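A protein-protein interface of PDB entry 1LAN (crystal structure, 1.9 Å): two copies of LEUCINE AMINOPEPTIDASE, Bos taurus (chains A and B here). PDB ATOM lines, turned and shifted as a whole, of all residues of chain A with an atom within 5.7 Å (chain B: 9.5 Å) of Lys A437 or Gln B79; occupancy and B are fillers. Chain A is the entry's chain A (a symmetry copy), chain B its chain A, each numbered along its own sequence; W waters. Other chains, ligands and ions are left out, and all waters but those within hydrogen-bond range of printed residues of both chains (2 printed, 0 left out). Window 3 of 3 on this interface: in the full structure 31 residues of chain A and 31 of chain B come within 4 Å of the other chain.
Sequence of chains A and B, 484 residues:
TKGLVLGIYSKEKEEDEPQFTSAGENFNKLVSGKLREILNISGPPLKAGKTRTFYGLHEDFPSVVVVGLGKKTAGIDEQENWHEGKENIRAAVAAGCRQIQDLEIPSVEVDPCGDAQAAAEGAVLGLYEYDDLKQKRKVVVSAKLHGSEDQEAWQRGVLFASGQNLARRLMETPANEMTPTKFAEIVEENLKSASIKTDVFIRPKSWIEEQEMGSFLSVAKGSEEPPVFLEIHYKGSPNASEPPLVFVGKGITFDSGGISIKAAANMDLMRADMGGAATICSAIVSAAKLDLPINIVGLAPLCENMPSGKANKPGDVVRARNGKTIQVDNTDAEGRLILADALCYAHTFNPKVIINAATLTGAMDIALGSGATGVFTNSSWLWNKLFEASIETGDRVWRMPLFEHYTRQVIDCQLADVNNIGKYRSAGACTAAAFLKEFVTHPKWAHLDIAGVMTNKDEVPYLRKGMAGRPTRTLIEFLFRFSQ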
ATOM      1  N   LEU A 402       5.192  23.840 -21.140  1.00  0.00           N
ATOM      2  CA  LEU A 402       3.907  24.431 -21.538  1.00  0.00           C
ATOM      3  C   LEU A 402       3.771  24.117 -23.033  1.00  0.00           C
ATOM      4  O   LEU A 402       4.008  24.983 -23.878  1.00  0.00           O
ATOM      5  CB  LEU A 402       3.901  25.951 -21.361  1.00  0.00           C
ATOM      6  CG  LEU A 402       3.171  26.610 -20.190  1.00  0.00           C
ATOM      7  CD1 LEU A 402       3.051  28.095 -20.517  1.00  0.00           C
ATOM      8  CD2 LEU A 402       1.780  26.008 -19.954  1.00  0.00           C
ATOM      9  N   PHE A 403       3.413  22.881 -23.360  1.00  0.00           N
ATOM     10  CA  PHE A 403       3.305  22.440 -24.752  1.00  0.00           C
ATOM     11  C   PHE A 403       1.848  22.314 -25.177  1.00  0.00           C
ATOM     12  O   PHE A 403       1.002  21.918 -24.367  1.00  0.00           O
ATOM     13  CB  PHE A 403       3.936  21.042 -24.909  1.00  0.00           C
ATOM     14  CG  PHE A 403       5.426  20.976 -24.695  1.00  0.00           C
ATOM     15  CD1 PHE A 403       6.227  22.107 -24.778  1.00  0.00           C
ATOM     16  CD2 PHE A 403       6.039  19.733 -24.486  1.00  0.00           C
ATOM     17  CE1 PHE A 403       7.622  22.008 -24.676  1.00  0.00           C
ATOM     18  CE2 PHE A 403       7.433  19.621 -24.385  1.00  0.00           C
ATOM     19  CZ  PHE A 403       8.225  20.761 -24.477  1.00  0.00           C
ATOM     20  N   GLU A 404       1.578  22.525 -26.467  1.00  0.00           N
ATOM     21  CA  GLU A 404       0.217  22.395 -26.997  1.00  0.00           C
ATOM     22  C   GLU A 404      -0.238  20.942 -26.837  1.00  0.00           C
ATOM     23  O   GLU A 404      -1.429  20.658 -26.767  1.00  0.00           O
ATOM     24  CB  GLU A 404       0.146  22.801 -28.477  1.00  0.00           C
ATOM     25  CG  GLU A 404      -1.287  22.800 -29.087  1.00  0.00           C
ATOM     26  CD  GLU A 404      -1.779  21.421 -29.572  1.00  0.00           C
ATOM     27  OE1 GLU A 404      -0.956  20.629 -30.079  1.00  0.00           O
ATOM     28  OE2 GLU A 404      -3.000  21.130 -29.456  1.00  0.00           O
ATOM     29  N   THR A 407      -2.468  20.916 -24.014  1.00  0.00           N
ATOM     30  CA  THR A 407      -3.681  21.707 -24.245  1.00  0.00           C
ATOM     31  C   THR A 407      -4.746  20.852 -24.940  1.00  0.00           C
ATOM     32  O   THR A 407      -5.940  20.955 -24.662  1.00  0.00           O
ATOM     33  CB  THR A 407      -3.375  22.901 -25.158  1.00  0.00           C
ATOM     34  OG1 THR A 407      -2.418  23.740 -24.520  1.00  0.00           O
ATOM     35  CG2 THR A 407      -4.649  23.702 -25.485  1.00  0.00           C
ATOM     36  N   ALA A 432      -2.976  20.657 -16.118  1.00  0.00           N
ATOM     37  CA  ALA A 432      -3.592  21.690 -15.265  1.00  0.00           C
ATOM     38  C   ALA A 432      -3.066  23.048 -15.725  1.00  0.00           C
ATOM     39  O   ALA A 432      -3.834  24.002 -15.907  1.00  0.00           O
ATOM     40  CB  ALA A 432      -3.255  21.454 -13.777  1.00  0.00           C
ATOM     41  N   ALA A 433      -1.755  23.111 -15.969  1.00  0.00           N
ATOM     42  CA  ALA A 433      -1.117  24.330 -16.454  1.00  0.00           C
ATOM     43  C   ALA A 433      -1.673  24.708 -17.841  1.00  0.00           C
ATOM     44  O   ALA A 433      -1.873  25.887 -18.139  1.00  0.00           O
ATOM     45  CB  ALA A 433       0.401  24.144 -16.519  1.00  0.00           C
ATOM     46  N   ALA A 434      -1.891  23.712 -18.698  1.00  0.00           N
ATOM     47  CA  ALA A 434      -2.450  23.960 -20.033  1.00  0.00           C
ATOM     48  C   ALA A 434      -3.841  24.564 -19.877  1.00  0.00           C
ATOM     49  O   ALA A 434      -4.195  25.505 -20.590  1.00  0.00           O
ATOM     50  CB  ALA A 434      -2.510  22.668 -20.839  1.00  0.00           C
ATOM     51  N   PHE A 435      -4.625  24.033 -18.936  1.00  0.00           N
ATOM     52  CA  PHE A 435      -5.970  24.546 -18.673  1.00  0.00           C
ATOM     53  C   PHE A 435      -5.877  26.042 -18.321  1.00  0.00           C
ATOM     54  O   PHE A 435      -6.644  26.859 -18.842  1.00  0.00           O
ATOM     55  CB  PHE A 435      -6.621  23.779 -17.497  1.00  0.00           C
ATOM     56  CG  PHE A 435      -8.004  24.268 -17.128  1.00  0.00           C
ATOM     57  CD1 PHE A 435      -8.174  25.404 -16.331  1.00  0.00           C
ATOM     58  CD2 PHE A 435      -9.141  23.601 -17.587  1.00  0.00           C
ATOM     59  CE1 PHE A 435      -9.455  25.869 -16.001  1.00  0.00           C
ATOM     60  CE2 PHE A 435     -10.430  24.064 -17.260  1.00  0.00           C
ATOM     61  CZ  PHE A 435     -10.585  25.196 -16.470  1.00  0.00           C
ATOM     62  N   LEU A 436      -4.943  26.408 -17.439  1.00  0.00           N
ATOM     63  CA  LEU A 436      -4.803  27.812 -17.037  1.00  0.00           C
ATOM     64  C   LEU A 436      -4.438  28.731 -18.202  1.00  0.00           C
ATOM     65  O   LEU A 436      -4.926  29.856 -18.283  1.00  0.00           O
ATOM     66  CB  LEU A 436      -3.782  27.961 -15.898  1.00  0.00           C
ATOM     67  CG  LEU A 436      -4.073  27.248 -14.567  1.00  0.00           C
ATOM     68  CD1 LEU A 436      -2.874  27.402 -13.636  1.00  0.00           C
ATOM     69  CD2 LEU A 436      -5.340  27.819 -13.926  1.00  0.00           C
ATOM     70  N   LYS A 437      -3.633  28.223 -19.129  1.00  0.00           N
ATOM     71  CA  LYS A 437      -3.185  28.990 -20.290  1.00  0.00           C
ATOM     72  C   LYS A 437      -4.349  29.452 -21.177  1.00  0.00           C
ATOM     73  O   LYS A 437      -4.254  30.470 -21.862  1.00  0.00           O
ATOM     74  CB  LYS A 437      -2.199  28.163 -21.125  1.00  0.00           C
ATOM     75  CG  LYS A 437      -1.146  28.994 -21.846  1.00  0.00           C
ATOM     76  CD  LYS A 437      -0.722  28.387 -23.202  1.00  0.00           C
ATOM     77  CE  LYS A 437      -0.138  26.969 -23.126  1.00  0.00           C
ATOM     78  NZ  LYS A 437       0.363  26.491 -24.467  1.00  0.00           N
ATOM     79  N   GLU A 438      -5.456  28.717 -21.142  1.00  0.00           N
ATOM     80  CA  GLU A 438      -6.639  29.073 -21.917  1.00  0.00           C
ATOM     81  C   GLU A 438      -7.283  30.340 -21.380  1.00  0.00           C
ATOM     82  O   GLU A 438      -8.190  30.893 -22.001  1.00  0.00           O
ATOM     83  CB  GLU A 438      -7.667  27.934 -21.899  1.00  0.00           C
ATOM     84  CG  GLU A 438      -7.174  26.659 -22.550  1.00  0.00           C
ATOM     85  CD  GLU A 438      -6.685  26.909 -23.950  1.00  0.00           C
ATOM     86  OE1 GLU A 438      -7.503  27.333 -24.794  1.00  0.00           O
ATOM     87  OE2 GLU A 438      -5.478  26.714 -24.210  1.00  0.00           O
ATOM     88  N   PHE A 439      -6.819  30.802 -20.226  1.00  0.00           N
ATOM     89  CA  PHE A 439      -7.375  32.007 -19.621  1.00  0.00           C
ATOM     90  C   PHE A 439      -6.321  33.109 -19.542  1.00  0.00           C
ATOM     91  O   PHE A 439      -6.497  34.125 -18.852  1.00  0.00           O
ATOM     92  CB  PHE A 439      -7.970  31.673 -18.242  1.00  0.00           C
ATOM     93  CG  PHE A 439      -9.126  30.704 -18.308  1.00  0.00           C
ATOM     94  CD1 PHE A 439     -10.419  31.159 -18.563  1.00  0.00           C
ATOM     95  CD2 PHE A 439      -8.909  29.328 -18.233  1.00  0.00           C
ATOM     96  CE1 PHE A 439     -11.475  30.261 -18.759  1.00  0.00           C
ATOM     97  CE2 PHE A 439      -9.967  28.417 -18.426  1.00  0.00           C
ATOM     98  CZ  PHE A 439     -11.251  28.891 -18.696  1.00  0.00           C
ATOM     99  N   VAL A 440      -5.249  32.939 -20.311  1.00  0.00           N
ATOM    100  CA  VAL A 440      -4.165  33.904 -20.326  1.00  0.00           C
ATOM    101  C   VAL A 440      -3.784  34.271 -21.759  1.00  0.00           C
ATOM    102  O   VAL A 440      -3.620  33.387 -22.599  1.00  0.00           O
ATOM    103  CB  VAL A 440      -2.892  33.313 -19.647  1.00  0.00           C
ATOM    104  CG1 VAL A 440      -1.713  34.265 -19.803  1.00  0.00           C
ATOM    105  CG2 VAL A 440      -3.155  33.022 -18.163  1.00  0.00           C
ATOM    106  N   THR A 441      -3.714  35.571 -22.047  1.00  0.00           N
ATOM    107  CA  THR A 441      -3.267  36.053 -23.359  1.00  0.00           C
ATOM    108  C   THR A 441      -2.015  36.931 -23.205  1.00  0.00           C
ATOM    109  O   THR A 441      -1.520  37.485 -24.172  1.00  0.00           O
ATOM    110  CB  THR A 441      -4.346  36.881 -24.083  1.00  0.00           C
ATOM    111  OG1 THR A 441      -4.673  38.019 -23.284  1.00  0.00           O
ATOM    112  CG2 THR A 441      -5.595  36.060 -24.325  1.00  0.00           C
ATOM    113  N   TRP A 445       3.748  35.389 -18.590  1.00  0.00           N
ATOM    114  CA  TRP A 445       2.983  34.751 -17.529  1.00  0.00           C
ATOM    115  C   TRP A 445       3.723  33.525 -17.000  1.00  0.00           C
ATOM    116  O   TRP A 445       4.259  32.743 -17.784  1.00  0.00           O
ATOM    117  CB  TRP A 445       1.596  34.335 -18.064  1.00  0.00           C
ATOM    118  CG  TRP A 445       0.870  33.326 -17.200  1.00  0.00           C
ATOM    119  CD1 TRP A 445       0.376  33.521 -15.939  1.00  0.00           C
ATOM    120  CD2 TRP A 445       0.598  31.948 -17.531  1.00  0.00           C
ATOM    121  NE1 TRP A 445      -0.178  32.354 -15.465  1.00  0.00           N
ATOM    122  CE2 TRP A 445      -0.057  31.374 -16.417  1.00  0.00           C
ATOM    123  CE3 TRP A 445       0.847  31.147 -18.659  1.00  0.00           C
ATOM    124  CZ2 TRP A 445      -0.469  30.032 -16.395  1.00  0.00           C
ATOM    125  CZ3 TRP A 445       0.437  29.804 -18.635  1.00  0.00           C
ATOM    126  CH2 TRP A 445      -0.214  29.268 -17.508  1.00  0.00           C
ATOM    127  N   GLY B  75       9.658  27.486 -38.733  1.00  0.00           N
ATOM    128  CA  GLY B  75      10.988  27.045 -38.370  1.00  0.00           C
ATOM    129  C   GLY B  75      10.949  26.602 -36.922  1.00  0.00           C
ATOM    130  O   GLY B  75       9.945  26.012 -36.484  1.00  0.00           O
ATOM    131  N   ILE B  76      12.007  26.890 -36.168  1.00  0.00           N
ATOM    132  CA  ILE B  76      12.070  26.517 -34.756  1.00  0.00           C
ATOM    133  C   ILE B  76      11.047  27.282 -33.914  1.00  0.00           C
ATOM    134  O   ILE B  76      10.976  28.521 -33.967  1.00  0.00           O
ATOM    135  CB  ILE B  76      13.474  26.741 -34.184  1.00  0.00           C
ATOM    136  CG1 ILE B  76      14.439  25.735 -34.812  1.00  0.00           C
ATOM    137  CG2 ILE B  76      13.457  26.610 -32.668  1.00  0.00           C
ATOM    138  CD1 ILE B  76      15.868  25.833 -34.284  1.00  0.00           C
ATOM    139  N   ASP B  77      10.224  26.528 -33.185  1.00  0.00           N
ATOM    140  CA  ASP B  77       9.197  27.093 -32.315  1.00  0.00           C
ATOM    141  C   ASP B  77       9.783  27.198 -30.923  1.00  0.00           C
ATOM    142  O   ASP B  77      10.039  26.194 -30.272  1.00  0.00           O
ATOM    143  CB  ASP B  77       7.943  26.215 -32.297  1.00  0.00           C
ATOM    144  CG  ASP B  77       6.778  26.862 -31.563  1.00  0.00           C
ATOM    145  OD1 ASP B  77       7.000  27.638 -30.612  1.00  0.00           O
ATOM    146  OD2 ASP B  77       5.621  26.596 -31.937  1.00  0.00           O
ATOM    147  N   GLU B  78       9.958  28.422 -30.456  1.00  0.00           N
ATOM    148  CA  GLU B  78      10.518  28.669 -29.145  1.00  0.00           C
ATOM    149  C   GLU B  78       9.646  28.134 -27.999  1.00  0.00           C
ATOM    150  O   GLU B  78      10.179  27.735 -26.973  1.00  0.00           O
ATOM    151  CB  GLU B  78      10.785  30.171 -28.979  1.00  0.00           C
ATOM    152  CG  GLU B  78      11.444  30.563 -27.657  1.00  0.00           C
ATOM    153  CD  GLU B  78      11.579  32.064 -27.491  1.00  0.00           C
ATOM    154  OE1 GLU B  78      11.094  32.816 -28.373  1.00  0.00           O
ATOM    155  OE2 GLU B  78      12.177  32.485 -26.464  1.00  0.00           O
ATOM    156  N   GLN B  79       8.325  28.117 -28.172  1.00  0.00           N
ATOM    157  CA  GLN B  79       7.414  27.606 -27.138  1.00  0.00           C
ATOM    158  C   GLN B  79       7.518  26.083 -27.027  1.00  0.00           C
ATOM    159  O   GLN B  79       7.604  25.533 -25.937  1.00  0.00           O
ATOM    160  CB  GLN B  79       5.940  27.955 -27.474  1.00  0.00           C
ATOM    161  CG  GLN B  79       4.895  27.623 -26.349  1.00  0.00           C
ATOM    162  CD  GLN B  79       3.520  27.080 -26.854  1.00  0.00           C
ATOM    163  OE1 GLN B  79       3.001  27.497 -27.892  1.00  0.00           O
ATOM    164  NE2 GLN B  79       2.941  26.151 -26.093  1.00  0.00           N
ATOM    165  N   GLU B  80       7.580  25.422 -28.176  1.00  0.00           N
ATOM    166  CA  GLU B  80       7.587  23.973 -28.233  1.00  0.00           C
ATOM    167  C   GLU B  80       8.937  23.260 -28.267  1.00  0.00           C
ATOM    168  O   GLU B  80       8.979  22.029 -28.264  1.00  0.00           O
ATOM    169  CB  GLU B  80       6.734  23.532 -29.426  1.00  0.00           C
ATOM    170  CG  GLU B  80       5.319  24.143 -29.453  1.00  0.00           C
ATOM    171  CD  GLU B  80       4.395  23.555 -28.399  1.00  0.00           C
ATOM    172  OE1 GLU B  80       4.700  22.472 -27.868  1.00  0.00           O
ATOM    173  OE2 GLU B  80       3.348  24.163 -28.108  1.00  0.00           O
ATOM    174  N   ASN B  81      10.026  24.016 -28.381  1.00  0.00           N
ATOM    175  CA  ASN B  81      11.364  23.426 -28.409  1.00  0.00           C
ATOM    176  C   ASN B  81      11.520  22.394 -29.541  1.00  0.00           C
ATOM    177  O   ASN B  81      12.044  21.293 -29.338  1.00  0.00           O
ATOM    178  CB  ASN B  81      11.710  22.774 -27.047  1.00  0.00           C
ATOM    179  CG  ASN B  81      11.789  23.777 -25.896  1.00  0.00           C
ATOM    180  OD1 ASN B  81      11.694  23.407 -24.709  1.00  0.00           O
ATOM    181  ND2 ASN B  81      11.985  25.040 -26.224  1.00  0.00           N
ATOM    182  N   TRP B  82      11.007  22.722 -30.723  1.00  0.00           N
ATOM    183  CA  TRP B  82      11.169  21.838 -31.871  1.00  0.00           C
ATOM    184  C   TRP B  82      11.033  22.599 -33.184  1.00  0.00           C
ATOM    185  O   TRP B  82      10.638  23.772 -33.204  1.00  0.00           O
ATOM    186  CB  TRP B  82      10.203  20.625 -31.828  1.00  0.00           C
ATOM    187  CG  TRP B  82       8.706  20.927 -31.973  1.00  0.00           C
ATOM    188  CD1 TRP B  82       8.128  22.101 -32.393  1.00  0.00           C
ATOM    189  CD2 TRP B  82       7.618  20.031 -31.690  1.00  0.00           C
ATOM    190  NE1 TRP B  82       6.759  21.984 -32.385  1.00  0.00           N
ATOM    191  CE2 TRP B  82       6.419  20.727 -31.960  1.00  0.00           C
ATOM    192  CE3 TRP B  82       7.542  18.700 -31.249  1.00  0.00           C
ATOM    193  CZ2 TRP B  82       5.156  20.148 -31.781  1.00  0.00           C
ATOM    194  CZ3 TRP B  82       6.288  18.125 -31.071  1.00  0.00           C
ATOM    195  CH2 TRP B  82       5.108  18.852 -31.349  1.00  0.00           C
ATOM    196  N   HIS B  83      11.405  21.947 -34.273  1.00  0.00           N
ATOM    197  CA  HIS B  83      11.262  22.561 -35.576  1.00  0.00           C
ATOM    198  C   HIS B  83       9.830  22.250 -36.019  1.00  0.00           C
ATOM    199  O   HIS B  83       9.513  21.121 -36.389  1.00  0.00           O
ATOM    200  CB  HIS B  83      12.269  21.956 -36.545  1.00  0.00           C
ATOM    201  CG  HIS B  83      12.342  22.680 -37.843  1.00  0.00           C
ATOM    202  ND1 HIS B  83      13.481  23.339 -38.261  1.00  0.00           N
ATOM    203  CD2 HIS B  83      11.406  22.900 -38.795  1.00  0.00           C
ATOM    204  CE1 HIS B  83      13.237  23.936 -39.416  1.00  0.00           C
ATOM    205  NE2 HIS B  83      11.988  23.686 -39.759  1.00  0.00           N
ATOM    206  N   GLU B  84       8.960  23.251 -35.968  1.00  0.00           N
ATOM    207  CA  GLU B  84       7.564  23.065 -36.341  1.00  0.00           C
ATOM    208  C   GLU B  84       7.351  22.580 -37.790  1.00  0.00           C
ATOM    209  O   GLU B  84       6.533  21.691 -38.040  1.00  0.00           O
ATOM    210  CB  GLU B  84       6.788  24.355 -36.089  1.00  0.00           C
ATOM    211  CG  GLU B  84       5.311  24.224 -36.348  1.00  0.00           C
ATOM    212  CD  GLU B  84       4.581  25.551 -36.275  1.00  0.00           C
ATOM    213  OE1 GLU B  84       5.205  26.570 -35.901  1.00  0.00           O
ATOM    214  OE2 GLU B  84       3.381  25.579 -36.610  1.00  0.00           O
ATOM    215  N   PHE B 387      19.450  18.017 -25.791  1.00  0.00           N
ATOM    216  CA  PHE B 387      18.381  18.974 -26.019  1.00  0.00           C
ATOM    217  C   PHE B 387      18.391  19.483 -27.464  1.00  0.00           C
ATOM    218  O   PHE B 387      17.346  19.512 -28.136  1.00  0.00           O
ATOM    219  CB  PHE B 387      18.490  20.142 -25.025  1.00  0.00           C
ATOM    220  CG  PHE B 387      17.423  21.187 -25.201  1.00  0.00           C
ATOM    221  CD1 PHE B 387      16.074  20.861 -25.072  1.00  0.00           C
ATOM    222  CD2 PHE B 387      17.766  22.501 -25.523  1.00  0.00           C
ATOM    223  CE1 PHE B 387      15.091  21.815 -25.263  1.00  0.00           C
ATOM    224  CE2 PHE B 387      16.788  23.466 -25.716  1.00  0.00           C
ATOM    225  CZ  PHE B 387      15.443  23.117 -25.585  1.00  0.00           C
ATOM    226  N   ILE B 391      15.468  18.986 -30.661  1.00  0.00           N
ATOM    227  CA  ILE B 391      14.788  20.082 -31.365  1.00  0.00           C
ATOM    228  C   ILE B 391      14.652  19.709 -32.850  1.00  0.00           C
ATOM    229  O   ILE B 391      13.604  19.939 -33.473  1.00  0.00           O
ATOM    230  CB  ILE B 391      15.560  21.448 -31.204  1.00  0.00           C
ATOM    231  CG1 ILE B 391      15.527  21.897 -29.741  1.00  0.00           C
ATOM    232  CG2 ILE B 391      14.932  22.543 -32.067  1.00  0.00           C
ATOM    233  CD1 ILE B 391      16.267  23.162 -29.482  1.00  0.00           C
ATOM    234  N   ARG B 396      11.101  15.154 -28.255  1.00  0.00           N
ATOM    235  CA  ARG B 396      11.573  15.969 -27.149  1.00  0.00           C
ATOM    236  C   ARG B 396      12.093  15.385 -25.831  1.00  0.00           C
ATOM    237  O   ARG B 396      11.693  14.291 -25.396  1.00  0.00           O
ATOM    238  CB  ARG B 396      10.521  17.039 -26.872  1.00  0.00           C
ATOM    239  CG  ARG B 396      10.086  17.786 -28.134  1.00  0.00           C
ATOM    240  CD  ARG B 396       9.019  18.834 -27.844  1.00  0.00           C
ATOM    241  NE  ARG B 396       7.673  18.265 -27.764  1.00  0.00           N
ATOM    242  CZ  ARG B 396       6.553  18.984 -27.774  1.00  0.00           C
ATOM    243  NH1 ARG B 396       6.608  20.308 -27.862  1.00  0.00           N
ATOM    244  NH2 ARG B 396       5.371  18.385 -27.706  1.00  0.00           N
ATOM    245  N   TRP B 398      13.322  16.727 -21.690  1.00  0.00           N
ATOM    246  CA  TRP B 398      13.093  17.773 -20.691  1.00  0.00           C
ATOM    247  C   TRP B 398      13.946  17.379 -19.488  1.00  0.00           C
ATOM    248  O   TRP B 398      13.907  16.225 -19.046  1.00  0.00           O
ATOM    249  CB  TRP B 398      11.596  17.833 -20.316  1.00  0.00           C
ATOM    250  CG  TRP B 398      11.202  19.092 -19.558  1.00  0.00           C
ATOM    251  CD1 TRP B 398      11.171  19.255 -18.193  1.00  0.00           C
ATOM    252  CD2 TRP B 398      10.893  20.371 -20.121  1.00  0.00           C
ATOM    253  NE1 TRP B 398      10.883  20.558 -17.876  1.00  0.00           N
ATOM    254  CE2 TRP B 398      10.700  21.268 -19.032  1.00  0.00           C
ATOM    255  CE3 TRP B 398      10.773  20.853 -21.437  1.00  0.00           C
ATOM    256  CZ2 TRP B 398      10.386  22.621 -19.223  1.00  0.00           C
ATOM    257  CZ3 TRP B 398      10.462  22.195 -21.624  1.00  0.00           C
ATOM    258  CH2 TRP B 398      10.268  23.067 -20.518  1.00  0.00           C
HETATM  259  O   HOH W   1       3.100  20.201 -28.257  1.00  0.00           O
HETATM  260  O   HOH W   2       6.033  27.623 -23.640  1.00  0.00           O
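The backbone carbonyl oxygen (O) of Leu A402 sits at hydrogen-bond distance from the side-chain amide nitrogen (NE2) of Gln B79 (2.7 Å). The side-chain amide nitrogen (NE2) of Gln B79 lies close to the side-chain amino group (NZ) of Lys A437 (3.1 Å). The side-chain carboxylate (OE2) of Glu B80 sits at hydrogen-bond distance from the backbone NH (N) of Glu A404 (2.9 Å).
The side-chain carboxylate (OD1) of Asp B77 lies within hydrogen-bond range of the backbone NH (N) of Gln B79, at 2.8 Å. The backbone NH of Glu B80 lies within hydrogen-bond range of the side-chain carboxylate of Asp B77 (3.3 Å). NE2 of Gln B79 lies within hydrogen-bond range of OE2 of Glu B80, 2.9 Å away. The guanidinium group (NH1) of Arg B396 is in salt-bridge range of the side-chain carboxylate (OE1) of Glu B80, 2.9 Å away.
Among the printed residues, merely in contact across the chains: Phe A403 with Glu B80, Phe A403 with Arg B396, Phe A403 with Gln B79, Glu A404 with Gln B79 and Phe A403 with Trp B398.
Lys A437 touches just one residue of chain B: Gln B79. Gln B79 touches just these residues of chain A: Leu A402, Phe A403, Glu A404 and Lys A437. No residue of chain B comes within 4 Å of Ala A434. No residue of chain B comes within 4 Å of Glu A438. No residue of chain B comes within 4 Å of Val A440. Printed residues of chain A within 4 Å of Glu B80: Phe A403 (3.4 Å) and Glu A404 (2.9 Å). Of the printed residues of chain A, Arg B396 touches Phe A403 (3.4 Å). Printed residues of chain B within 4 Å of Phe A403: Gln B79 (3.7 Å), Glu B80 (3.4 Å), Arg B396 (3.4 Å) and Trp B398 (3.9 Å). Of the printed residues of chain B, Leu A402 touches Gln B79 (2.7 Å). Ala A432 touches none of the printed residues of chain B. Thr A441 touches none of the printed residues of chain B.
Of the 15 printed residues of chain A, 4 touch a printed residue of chain B. Hydrophobic or aromatic side chains of chain A that line the printed part of chain B: Phe A403. Among the printed residues, 8 pairs touch across the chains. Among the printed residues, no Asp or Glu carboxylate lies within 4 Å of a Lys or Arg side-chain nitrogen of the other chain.
No position is printed for both chains.
Water W1 lies within hydrogen-bond range of OE1 of Glu B80 (2.8 Å), NH2 of Arg B396 (3.0 Å) and N of Glu A404 (3.3 Å). Water W2 bridges O of Leu A402 and O of Gln B79.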
